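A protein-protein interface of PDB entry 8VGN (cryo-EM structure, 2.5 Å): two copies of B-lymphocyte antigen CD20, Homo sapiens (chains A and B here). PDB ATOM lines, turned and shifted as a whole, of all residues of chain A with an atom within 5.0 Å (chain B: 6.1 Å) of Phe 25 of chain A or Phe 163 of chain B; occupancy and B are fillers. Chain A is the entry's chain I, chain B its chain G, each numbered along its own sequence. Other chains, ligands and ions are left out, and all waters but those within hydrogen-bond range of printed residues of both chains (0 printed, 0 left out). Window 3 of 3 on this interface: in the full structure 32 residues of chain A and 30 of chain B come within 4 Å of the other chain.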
ATOM      1  N   MET A  21       5.202 -13.414 -13.807  1.00  0.00           N
ATOM      2  CA  MET A  21       3.780 -13.505 -13.500  1.00  0.00           C
ATOM      3  C   MET A  21       3.459 -13.065 -12.073  1.00  0.00           C
ATOM      4  O   MET A  21       2.473 -12.358 -11.854  1.00  0.00           O
ATOM      5  CB  MET A  21       3.291 -14.923 -13.762  1.00  0.00           C
ATOM      6  CG  MET A  21       3.428 -15.357 -15.210  1.00  0.00           C
ATOM      7  SD  MET A  21       2.615 -14.268 -16.391  1.00  0.00           S
ATOM      8  CE  MET A  21       0.900 -14.526 -15.984  1.00  0.00           C
ATOM      9  N   ASN A  22       4.258 -13.477 -11.084  1.00  0.00           N
ATOM     10  CA  ASN A  22       4.075 -12.941  -9.733  1.00  0.00           C
ATOM     11  C   ASN A  22       4.192 -11.425  -9.695  1.00  0.00           C
ATOM     12  O   ASN A  22       3.448 -10.760  -8.970  1.00  0.00           O
ATOM     13  CB  ASN A  22       5.095 -13.534  -8.762  1.00  0.00           C
ATOM     14  CG  ASN A  22       4.697 -14.882  -8.243  1.00  0.00           C
ATOM     15  OD1 ASN A  22       3.522 -15.152  -8.026  1.00  0.00           O
ATOM     16  ND2 ASN A  22       5.682 -15.734  -8.002  1.00  0.00           N
ATOM     17  N   GLY A  23       5.111 -10.863 -10.470  1.00  0.00           N
ATOM     18  CA  GLY A  23       5.233  -9.416 -10.527  1.00  0.00           C
ATOM     19  C   GLY A  23       4.013  -8.732 -11.105  1.00  0.00           C
ATOM     20  O   GLY A  23       3.535  -7.732 -10.570  1.00  0.00           O
ATOM     21  N   LEU A  24       3.500  -9.260 -12.210  1.00  0.00           N
ATOM     22  CA  LEU A  24       2.289  -8.721 -12.821  1.00  0.00           C
ATOM     23  C   LEU A  24       1.064  -8.875 -11.929  1.00  0.00           C
ATOM     24  O   LEU A  24       0.222  -7.976 -11.876  1.00  0.00           O
ATOM     25  CB  LEU A  24       2.058  -9.398 -14.166  1.00  0.00           C
ATOM     26  CG  LEU A  24       3.154  -9.130 -15.193  1.00  0.00           C
ATOM     27  CD1 LEU A  24       2.921  -9.949 -16.434  1.00  0.00           C
ATOM     28  CD2 LEU A  24       3.235  -7.658 -15.522  1.00  0.00           C
ATOM     29  N   PHE A  25       0.944  -9.992 -11.215  1.00  0.00           N
ATOM     30  CA  PHE A  25      -0.144 -10.132 -10.248  1.00  0.00           C
ATOM     31  C   PHE A  25      -0.056  -9.113  -9.116  1.00  0.00           C
ATOM     32  O   PHE A  25      -1.076  -8.558  -8.698  1.00  0.00           O
ATOM     33  CB  PHE A  25      -0.164 -11.541  -9.655  1.00  0.00           C
ATOM     34  CG  PHE A  25      -0.317 -12.642 -10.666  1.00  0.00           C
ATOM     35  CD1 PHE A  25      -0.764 -12.388 -11.945  1.00  0.00           C
ATOM     36  CD2 PHE A  25      -0.016 -13.947 -10.322  1.00  0.00           C
ATOM     37  CE1 PHE A  25      -0.900 -13.413 -12.857  1.00  0.00           C
ATOM     38  CE2 PHE A  25      -0.154 -14.965 -11.230  1.00  0.00           C
ATOM     39  CZ  PHE A  25      -0.593 -14.695 -12.495  1.00  0.00           C
ATOM     40  N   HIS A  26       1.145  -8.850  -8.605  1.00  0.00           N
ATOM     41  CA  HIS A  26       1.313  -7.802  -7.599  1.00  0.00           C
ATOM     42  C   HIS A  26       0.916  -6.432  -8.123  1.00  0.00           C
ATOM     43  O   HIS A  26       0.238  -5.669  -7.432  1.00  0.00           O
ATOM     44  CB  HIS A  26       2.749  -7.780  -7.098  1.00  0.00           C
ATOM     45  CG  HIS A  26       3.016  -8.768  -6.015  1.00  0.00           C
ATOM     46  ND1 HIS A  26       3.167 -10.114  -6.255  1.00  0.00           N
ATOM     47  CD2 HIS A  26       3.160  -8.605  -4.681  1.00  0.00           C
ATOM     48  CE1 HIS A  26       3.389 -10.739  -5.115  1.00  0.00           C
ATOM     49  NE2 HIS A  26       3.390  -9.846  -4.145  1.00  0.00           N
ATOM     50  N   ILE A  27       1.353  -6.089  -9.331  1.00  0.00           N
ATOM     51  CA  ILE A  27       0.978  -4.806  -9.911  1.00  0.00           C
ATOM     52  C   ILE A  27      -0.533  -4.703 -10.072  1.00  0.00           C
ATOM     53  O   ILE A  27      -1.136  -3.670  -9.759  1.00  0.00           O
ATOM     54  CB  ILE A  27       1.716  -4.595 -11.244  1.00  0.00           C
ATOM     55  CG1 ILE A  27       3.207  -4.400 -10.984  1.00  0.00           C
ATOM     56  CG2 ILE A  27       1.154  -3.411 -11.984  1.00  0.00           C
ATOM     57  CD1 ILE A  27       4.068  -4.586 -12.195  1.00  0.00           C
ATOM     58  N   ALA A  28      -1.173  -5.770 -10.547  1.00  0.00           N
ATOM     59  CA  ALA A  28      -2.624  -5.768 -10.693  1.00  0.00           C
ATOM     60  C   ALA A  28      -3.341  -5.686  -9.351  1.00  0.00           C
ATOM     61  O   ALA A  28      -4.260  -4.881  -9.181  1.00  0.00           O
ATOM     62  CB  ALA A  28      -3.068  -7.012 -11.457  1.00  0.00           C
ATOM     63  N   LEU A  29      -2.940  -6.510  -8.383  1.00  0.00           N
ATOM     64  CA  LEU A  29      -3.507  -6.408  -7.040  1.00  0.00           C
ATOM     65  C   LEU A  29      -3.230  -5.057  -6.400  1.00  0.00           C
ATOM     66  O   LEU A  29      -4.059  -4.545  -5.646  1.00  0.00           O
ATOM     67  CB  LEU A  29      -2.981  -7.526  -6.147  1.00  0.00           C
ATOM     68  CG  LEU A  29      -3.405  -8.943  -6.509  1.00  0.00           C
ATOM     69  CD1 LEU A  29      -2.566  -9.942  -5.747  1.00  0.00           C
ATOM     70  CD2 LEU A  29      -4.876  -9.141  -6.230  1.00  0.00           C
ATOM     71  N   GLY A  30      -2.069  -4.470  -6.673  1.00  0.00           N
ATOM     72  CA  GLY A  30      -1.784  -3.151  -6.134  1.00  0.00           C
ATOM     73  C   GLY A  30      -2.693  -2.067  -6.678  1.00  0.00           C
ATOM     74  O   GLY A  30      -3.298  -1.314  -5.914  1.00  0.00           O
ATOM     75  N   PHE A 163       0.808 -14.820  -2.800  1.00  0.00           N
ATOM     76  CA  PHE A 163       1.729 -14.649  -3.921  1.00  0.00           C
ATOM     77  C   PHE A 163       3.053 -13.999  -3.533  1.00  0.00           C
ATOM     78  O   PHE A 163       4.074 -14.277  -4.167  1.00  0.00           O
ATOM     79  CB  PHE A 163       1.042 -13.874  -5.040  1.00  0.00           C
ATOM     80  CG  PHE A 163       0.019 -14.684  -5.766  1.00  0.00           C
ATOM     81  CD1 PHE A 163       0.407 -15.756  -6.543  1.00  0.00           C
ATOM     82  CD2 PHE A 163      -1.323 -14.409  -5.644  1.00  0.00           C
ATOM     83  CE1 PHE A 163      -0.521 -16.520  -7.199  1.00  0.00           C
ATOM     84  CE2 PHE A 163      -2.254 -15.174  -6.300  1.00  0.00           C
ATOM     85  CZ  PHE A 163      -1.852 -16.228  -7.076  1.00  0.00           C
ATOM     86  N   VAL B  18       3.538 -20.065 -17.447  1.00  0.00           N
ATOM     87  CA  VAL B  18       2.673 -18.896 -17.574  1.00  0.00           C
ATOM     88  C   VAL B  18       1.197 -19.267 -17.479  1.00  0.00           C
ATOM     89  O   VAL B  18       0.416 -18.584 -16.807  1.00  0.00           O
ATOM     90  CB  VAL B  18       2.984 -18.165 -18.892  1.00  0.00           C
ATOM     91  CG1 VAL B  18       1.910 -17.166 -19.205  1.00  0.00           C
ATOM     92  CG2 VAL B  18       4.316 -17.482 -18.801  1.00  0.00           C
ATOM     93  N   MET B  21       0.226 -20.138 -13.859  1.00  0.00           N
ATOM     94  CA  MET B  21       0.068 -18.886 -13.130  1.00  0.00           C
ATOM     95  C   MET B  21      -1.213 -18.145 -13.509  1.00  0.00           C
ATOM     96  O   MET B  21      -1.910 -17.632 -12.631  1.00  0.00           O
ATOM     97  CB  MET B  21       1.298 -18.013 -13.340  1.00  0.00           C
ATOM     98  CG  MET B  21       2.559 -18.619 -12.753  1.00  0.00           C
ATOM     99  SD  MET B  21       2.450 -18.913 -10.981  1.00  0.00           S
ATOM    100  CE  MET B  21       2.711 -17.275 -10.339  1.00  0.00           C
ATOM    101  N   ASN B  22      -1.537 -18.049 -14.803  1.00  0.00           N
ATOM    102  CA  ASN B  22      -2.831 -17.478 -15.184  1.00  0.00           C
ATOM    103  C   ASN B  22      -3.995 -18.233 -14.562  1.00  0.00           C
ATOM    104  O   ASN B  22      -4.985 -17.624 -14.149  1.00  0.00           O
ATOM    105  CB  ASN B  22      -3.011 -17.475 -16.701  1.00  0.00           C
ATOM    106  CG  ASN B  22      -2.307 -16.339 -17.379  1.00  0.00           C
ATOM    107  OD1 ASN B  22      -2.182 -15.254 -16.823  1.00  0.00           O
ATOM    108  ND2 ASN B  22      -1.866 -16.569 -18.606  1.00  0.00           N
ATOM    109  N   LEU B  24      -3.976 -20.037 -11.637  1.00  0.00           N
ATOM    110  CA  LEU B  24      -3.998 -19.731 -10.211  1.00  0.00           C
ATOM    111  C   LEU B  24      -4.520 -18.334  -9.924  1.00  0.00           C
ATOM    112  O   LEU B  24      -5.256 -18.130  -8.955  1.00  0.00           O
ATOM    113  CB  LEU B  24      -2.599 -19.898  -9.631  1.00  0.00           C
ATOM    114  CG  LEU B  24      -2.074 -21.327  -9.621  1.00  0.00           C
ATOM    115  CD1 LEU B  24      -0.642 -21.349  -9.163  1.00  0.00           C
ATOM    116  CD2 LEU B  24      -2.939 -22.198  -8.743  1.00  0.00           C
ATOM    117  N   PHE B  25      -4.165 -17.358 -10.750  1.00  0.00           N
ATOM    118  CA  PHE B  25      -4.673 -16.010 -10.532  1.00  0.00           C
ATOM    119  C   PHE B  25      -6.147 -15.857 -10.895  1.00  0.00           C
ATOM    120  O   PHE B  25      -6.847 -15.055 -10.272  1.00  0.00           O
ATOM    121  CB  PHE B  25      -3.827 -15.010 -11.305  1.00  0.00           C
ATOM    122  CG  PHE B  25      -3.900 -13.623 -10.759  1.00  0.00           C
ATOM    123  CD1 PHE B  25      -3.548 -13.373  -9.446  1.00  0.00           C
ATOM    124  CD2 PHE B  25      -4.289 -12.566 -11.551  1.00  0.00           C
ATOM    125  CE1 PHE B  25      -3.598 -12.106  -8.931  1.00  0.00           C
ATOM    126  CE2 PHE B  25      -4.337 -11.292 -11.035  1.00  0.00           C
ATOM    127  CZ  PHE B  25      -3.992 -11.065  -9.725  1.00  0.00           C
ATOM    128  N   HIS B  26      -6.644 -16.597 -11.886  1.00  0.00           N
ATOM    129  CA  HIS B  26      -8.089 -16.671 -12.088  1.00  0.00           C
ATOM    130  C   HIS B  26      -8.807 -17.237 -10.876  1.00  0.00           C
ATOM    131  O   HIS B  26      -9.855 -16.723 -10.475  1.00  0.00           O
ATOM    132  CB  HIS B  26      -8.412 -17.505 -13.319  1.00  0.00           C
ATOM    133  CG  HIS B  26      -8.392 -16.728 -14.590  1.00  0.00           C
ATOM    134  ND1 HIS B  26      -7.227 -16.342 -15.210  1.00  0.00           N
ATOM    135  CD2 HIS B  26      -9.400 -16.263 -15.360  1.00  0.00           C
ATOM    136  CE1 HIS B  26      -7.518 -15.670 -16.307  1.00  0.00           C
ATOM    137  NE2 HIS B  26      -8.830 -15.608 -16.422  1.00  0.00           N
ATOM    138  N   LEU B  29      -8.665 -14.440  -8.192  1.00  0.00           N
ATOM    139  CA  LEU B  29      -9.638 -13.405  -8.533  1.00  0.00           C
ATOM    140  C   LEU B  29     -11.072 -13.898  -8.438  1.00  0.00           C
ATOM    141  O   LEU B  29     -11.964 -13.127  -8.080  1.00  0.00           O
ATOM    142  CB  LEU B  29      -9.380 -12.862  -9.934  1.00  0.00           C
ATOM    143  CG  LEU B  29      -8.091 -12.079 -10.143  1.00  0.00           C
ATOM    144  CD1 LEU B  29      -7.853 -11.878 -11.620  1.00  0.00           C
ATOM    145  CD2 LEU B  29      -8.151 -10.756  -9.416  1.00  0.00           C
ATOM    146  N   TYR B  57      -6.546 -23.850 -17.334  1.00  0.00           N
ATOM    147  CA  TYR B  57      -5.217 -23.339 -17.644  1.00  0.00           C
ATOM    148  C   TYR B  57      -4.129 -24.088 -16.890  1.00  0.00           C
ATOM    149  O   TYR B  57      -3.036 -24.287 -17.426  1.00  0.00           O
ATOM    150  CB  TYR B  57      -5.128 -21.852 -17.327  1.00  0.00           C
ATOM    151  CG  TYR B  57      -6.267 -21.030 -17.864  1.00  0.00           C
ATOM    152  CD1 TYR B  57      -6.896 -21.359 -19.051  1.00  0.00           C
ATOM    153  CD2 TYR B  57      -6.709 -19.915 -17.180  1.00  0.00           C
ATOM    154  CE1 TYR B  57      -7.919 -20.593 -19.541  1.00  0.00           C
ATOM    155  CE2 TYR B  57      -7.739 -19.159 -17.653  1.00  0.00           C
ATOM    156  CZ  TYR B  57      -8.336 -19.494 -18.836  1.00  0.00           C
ATOM    157  OH  TYR B  57      -9.387 -18.742 -19.287  1.00  0.00           O
ATOM    158  N   SER B 158     -12.022  -6.299 -14.760  1.00  0.00           N
ATOM    159  CA  SER B 158     -11.097  -5.877 -15.804  1.00  0.00           C
ATOM    160  C   SER B 158      -9.681  -6.414 -15.617  1.00  0.00           C
ATOM    161  O   SER B 158      -8.965  -6.592 -16.604  1.00  0.00           O
ATOM    162  CB  SER B 158     -11.073  -4.355 -15.887  1.00  0.00           C
ATOM    163  OG  SER B 158     -10.776  -3.786 -14.633  1.00  0.00           O
ATOM    164  N   VAL B 159      -9.248  -6.664 -14.383  1.00  0.00           N
ATOM    165  CA  VAL B 159      -8.039  -7.459 -14.170  1.00  0.00           C
ATOM    166  C   VAL B 159      -8.224  -8.881 -14.685  1.00  0.00           C
ATOM    167  O   VAL B 159      -7.344  -9.440 -15.347  1.00  0.00           O
ATOM    168  CB  VAL B 159      -7.641  -7.453 -12.685  1.00  0.00           C
ATOM    169  CG1 VAL B 159      -6.559  -8.470 -12.430  1.00  0.00           C
ATOM    170  CG2 VAL B 159      -7.158  -6.081 -12.278  1.00  0.00           C
ATOM    171  N   MET B 160      -9.360  -9.495 -14.378  1.00  0.00           N
ATOM    172  CA  MET B 160      -9.631 -10.838 -14.882  1.00  0.00           C
ATOM    173  C   MET B 160      -9.741 -10.875 -16.401  1.00  0.00           C
ATOM    174  O   MET B 160      -9.325 -11.849 -17.035  1.00  0.00           O
ATOM    175  CB  MET B 160     -10.902 -11.383 -14.243  1.00  0.00           C
ATOM    176  CG  MET B 160     -11.185 -12.820 -14.597  1.00  0.00           C
ATOM    177  SD  MET B 160     -12.268 -13.606 -13.403  1.00  0.00           S
ATOM    178  CE  MET B 160     -13.720 -12.586 -13.584  1.00  0.00           C
ATOM    179  N   LEU B 161     -10.296  -9.828 -17.005  1.00  0.00           N
ATOM    180  CA  LEU B 161     -10.332  -9.729 -18.461  1.00  0.00           C
ATOM    181  C   LEU B 161      -8.943  -9.726 -19.086  1.00  0.00           C
ATOM    182  O   LEU B 161      -8.690 -10.457 -20.046  1.00  0.00           O
ATOM    183  CB  LEU B 161     -11.099  -8.473 -18.873  1.00  0.00           C
ATOM    184  CG  LEU B 161     -11.528  -8.220 -20.322  1.00  0.00           C
ATOM    185  CD1 LEU B 161     -12.473  -7.051 -20.323  1.00  0.00           C
ATOM    186  CD2 LEU B 161     -10.392  -7.934 -21.276  1.00  0.00           C
ATOM    187  N   ILE B 162      -8.034  -8.895 -18.580  1.00  0.00           N
ATOM    188  CA  ILE B 162      -6.710  -8.826 -19.195  1.00  0.00           C
ATOM    189  C   ILE B 162      -5.905 -10.114 -19.025  1.00  0.00           C
ATOM    190  O   ILE B 162      -5.133 -10.482 -19.916  1.00  0.00           O
ATOM    191  CB  ILE B 162      -5.946  -7.592 -18.674  1.00  0.00           C
ATOM    192  CG1 ILE B 162      -4.639  -7.415 -19.436  1.00  0.00           C
ATOM    193  CG2 ILE B 162      -5.657  -7.691 -17.209  1.00  0.00           C
ATOM    194  CD1 ILE B 162      -4.031  -6.050 -19.272  1.00  0.00           C
ATOM    195  N   PHE B 163      -6.062 -10.827 -17.912  1.00  0.00           N
ATOM    196  CA  PHE B 163      -5.428 -12.138 -17.797  1.00  0.00           C
ATOM    197  C   PHE B 163      -6.150 -13.239 -18.566  1.00  0.00           C
ATOM    198  O   PHE B 163      -5.508 -14.198 -18.998  1.00  0.00           O
ATOM    199  CB  PHE B 163      -5.274 -12.504 -16.324  1.00  0.00           C
ATOM    200  CG  PHE B 163      -4.202 -11.722 -15.640  1.00  0.00           C
ATOM    201  CD1 PHE B 163      -2.878 -11.926 -15.967  1.00  0.00           C
ATOM    202  CD2 PHE B 163      -4.512 -10.759 -14.710  1.00  0.00           C
ATOM    203  CE1 PHE B 163      -1.887 -11.199 -15.361  1.00  0.00           C
ATOM    204  CE2 PHE B 163      -3.520 -10.029 -14.105  1.00  0.00           C
ATOM    205  CZ  PHE B 163      -2.209 -10.251 -14.430  1.00  0.00           C
ATOM    206  N   ALA B 164      -7.461 -13.126 -18.759  1.00  0.00           N
ATOM    207  CA  ALA B 164      -8.148 -14.000 -19.706  1.00  0.00           C
ATOM    208  C   ALA B 164      -7.686 -13.754 -21.136  1.00  0.00           C
ATOM    209  O   ALA B 164      -7.504 -14.698 -21.909  1.00  0.00           O
ATOM    210  CB  ALA B 164      -9.657 -13.805 -19.599  1.00  0.00           C
ATOM    211  N   PHE B 165      -7.496 -12.492 -21.502  1.00  0.00           N
ATOM    212  CA  PHE B 165      -6.941 -12.144 -22.804  1.00  0.00           C
ATOM    213  C   PHE B 165      -5.495 -12.606 -22.953  1.00  0.00           C
ATOM    214  O   PHE B 165      -5.073 -12.993 -24.046  1.00  0.00           O
ATOM    215  CB  PHE B 165      -7.047 -10.633 -22.992  1.00  0.00           C
ATOM    216  CG  PHE B 165      -6.498 -10.133 -24.287  1.00  0.00           C
ATOM    217  CD1 PHE B 165      -6.848 -10.735 -25.475  1.00  0.00           C
ATOM    218  CD2 PHE B 165      -5.646  -9.050 -24.319  1.00  0.00           C
ATOM    219  CE1 PHE B 165      -6.367 -10.265 -26.670  1.00  0.00           C
ATOM    220  CE2 PHE B 165      -5.150  -8.582 -25.513  1.00  0.00           C
ATOM    221  CZ  PHE B 165      -5.509  -9.192 -26.690  1.00  0.00           C
ATOM    222  N   PHE B 166      -4.717 -12.557 -21.872  1.00  0.00           N
ATOM    223  CA  PHE B 166      -3.376 -13.140 -21.866  1.00  0.00           C
ATOM    224  C   PHE B 166      -3.385 -14.626 -22.221  1.00  0.00           C
ATOM    225  O   PHE B 166      -2.623 -15.067 -23.084  1.00  0.00           O
ATOM    226  CB  PHE B 166      -2.747 -12.915 -20.490  1.00  0.00           C
ATOM    227  CG  PHE B 166      -1.244 -12.985 -20.468  1.00  0.00           C
ATOM    228  CD1 PHE B 166      -0.565 -14.043 -21.039  1.00  0.00           C
ATOM    229  CD2 PHE B 166      -0.511 -11.994 -19.848  1.00  0.00           C
ATOM    230  CE1 PHE B 166       0.807 -14.109 -21.006  1.00  0.00           C
ATOM    231  CE2 PHE B 166       0.870 -12.055 -19.812  1.00  0.00           C
ATOM    232  CZ  PHE B 166       1.527 -13.116 -20.395  1.00  0.00           C
ATOM    233  N   GLN B 167      -4.252 -15.410 -21.579  1.00  0.00           N
ATOM    234  CA  GLN B 167      -4.389 -16.822 -21.929  1.00  0.00           C
ATOM    235  C   GLN B 167      -4.728 -17.027 -23.398  1.00  0.00           C
ATOM    236  O   GLN B 167      -4.140 -17.881 -24.066  1.00  0.00           O
ATOM    237  CB  GLN B 167      -5.444 -17.488 -21.052  1.00  0.00           C
ATOM    238  CG  GLN B 167      -4.880 -18.092 -19.807  1.00  0.00           C
ATOM    239  CD  GLN B 167      -3.811 -19.120 -20.112  1.00  0.00           C
ATOM    240  OE1 GLN B 167      -2.626 -18.871 -19.910  1.00  0.00           O
ATOM    241  NE2 GLN B 167      -4.222 -20.281 -20.591  1.00  0.00           N
ATOM    242  N   GLU B 168      -5.684 -16.264 -23.914  1.00  0.00           N
ATOM    243  CA  GLU B 168      -6.106 -16.430 -25.299  1.00  0.00           C
ATOM    244  C   GLU B 168      -4.934 -16.274 -26.261  1.00  0.00           C
ATOM    245  O   GLU B 168      -4.773 -17.069 -27.190  1.00  0.00           O
ATOM    246  CB  GLU B 168      -7.219 -15.430 -25.603  1.00  0.00           C
ATOM    247  CG  GLU B 168      -8.025 -15.700 -26.855  1.00  0.00           C
ATOM    248  CD  GLU B 168      -7.302 -15.296 -28.118  1.00  0.00           C
ATOM    249  OE1 GLU B 168      -6.551 -14.301 -28.080  1.00  0.00           O
ATOM    250  OE2 GLU B 168      -7.491 -15.966 -29.153  1.00  0.00           O
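O of Asn 22 of chain A is in hydrogen-bond range of ND1 of His 26 of chain A, 2.8 Å away.
OE1 of Gln 167 of chain B is in hydrogen-bond range of ND2 of Asn 22 of chain B (2.8 Å).
O of Asn 22 of chain B lies within hydrogen-bond range of ND1 of His 26 of chain B (2.8 Å).
Met 21 of chain A touches Met 21 of chain B.
CE of Met 21 of chain A touches OD1 of Asn 22 of chain B (3.3 Å).
Asn 22 of chain A touches Met 21 of chain B.
Phe 25 of chain A touches Met 21 of chain B.
Phe 25 of chain B touches Phe 25 of chain A.
Phe 25 of chain A touches Phe 163 of chain B.
CB of Ala 28 of chain A touches CG1 of Val 159 of chain B, at 3.9 Å.
CG of Leu 29 of chain A touches CZ of Phe 25 of chain B, at 3.9 Å.
Phe 163 of chain A touches Phe 25 of chain B (CE2 to CD1, 3.8 Å).
Phe 25 of chain A touches three residues of chain B.
Phe 163 of chain B touches one residue of chain A.
Of the printed residues of chain A, Val 159 of chain B touches Ala 28.
Of the printed residues of chain B, Asn 22 of chain A touches Met 21.
The nearest residue of chain B that does not touch Phe 25 of chain A is Asn 22 of chain B (4.2 Å).
The nearest residue of chain A that does not touch Phe 163 of chain B is Ala 28 of chain A (4.04 Å).
The nearest printed residue of chain B that does not touch Leu 29 of chain A is Leu 29 of chain B (4.8 Å).
Printed residues of chain B that touch a printed residue of chain A: Met 21, Asn 22, Phe 25, Val 159 and Phe 163.
Printed residues of chain A that touch a printed residue of chain B: Met 21, Asn 22, Phe 25, Ala 28, Leu 29 and Phe 163.
Hydrophobic or aromatic side chains of chain A within 4 Å of the printed part of chain B: Met 21, Phe 25, Ala 28, Leu 29 and Phe 163.
Among the printed residues, no Asp or Glu carboxylate lies within 4 Å of a Lys or Arg side-chain nitrogen of the other chain.
Met 21 of chain A touches its own counterpart, Met 21 of chain B.
Met 21 of chain A touches Asn 22 of chain B, and with the chains exchanged Asn 22 of chain A touches Met 21 of chain B.
Phe 25 of chain B touches its own counterpart, Phe 25 of chain A.
Phe 25 of chain A touches Phe 163 of chain B, and with the chains exchanged Phe 163 of chain A touches Phe 25 of chain B.
7 positions are printed for both chains.
Of the 9 pairs that touch across the chains among the printed residues, 6 have their exchanged pair printed and touching as well.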
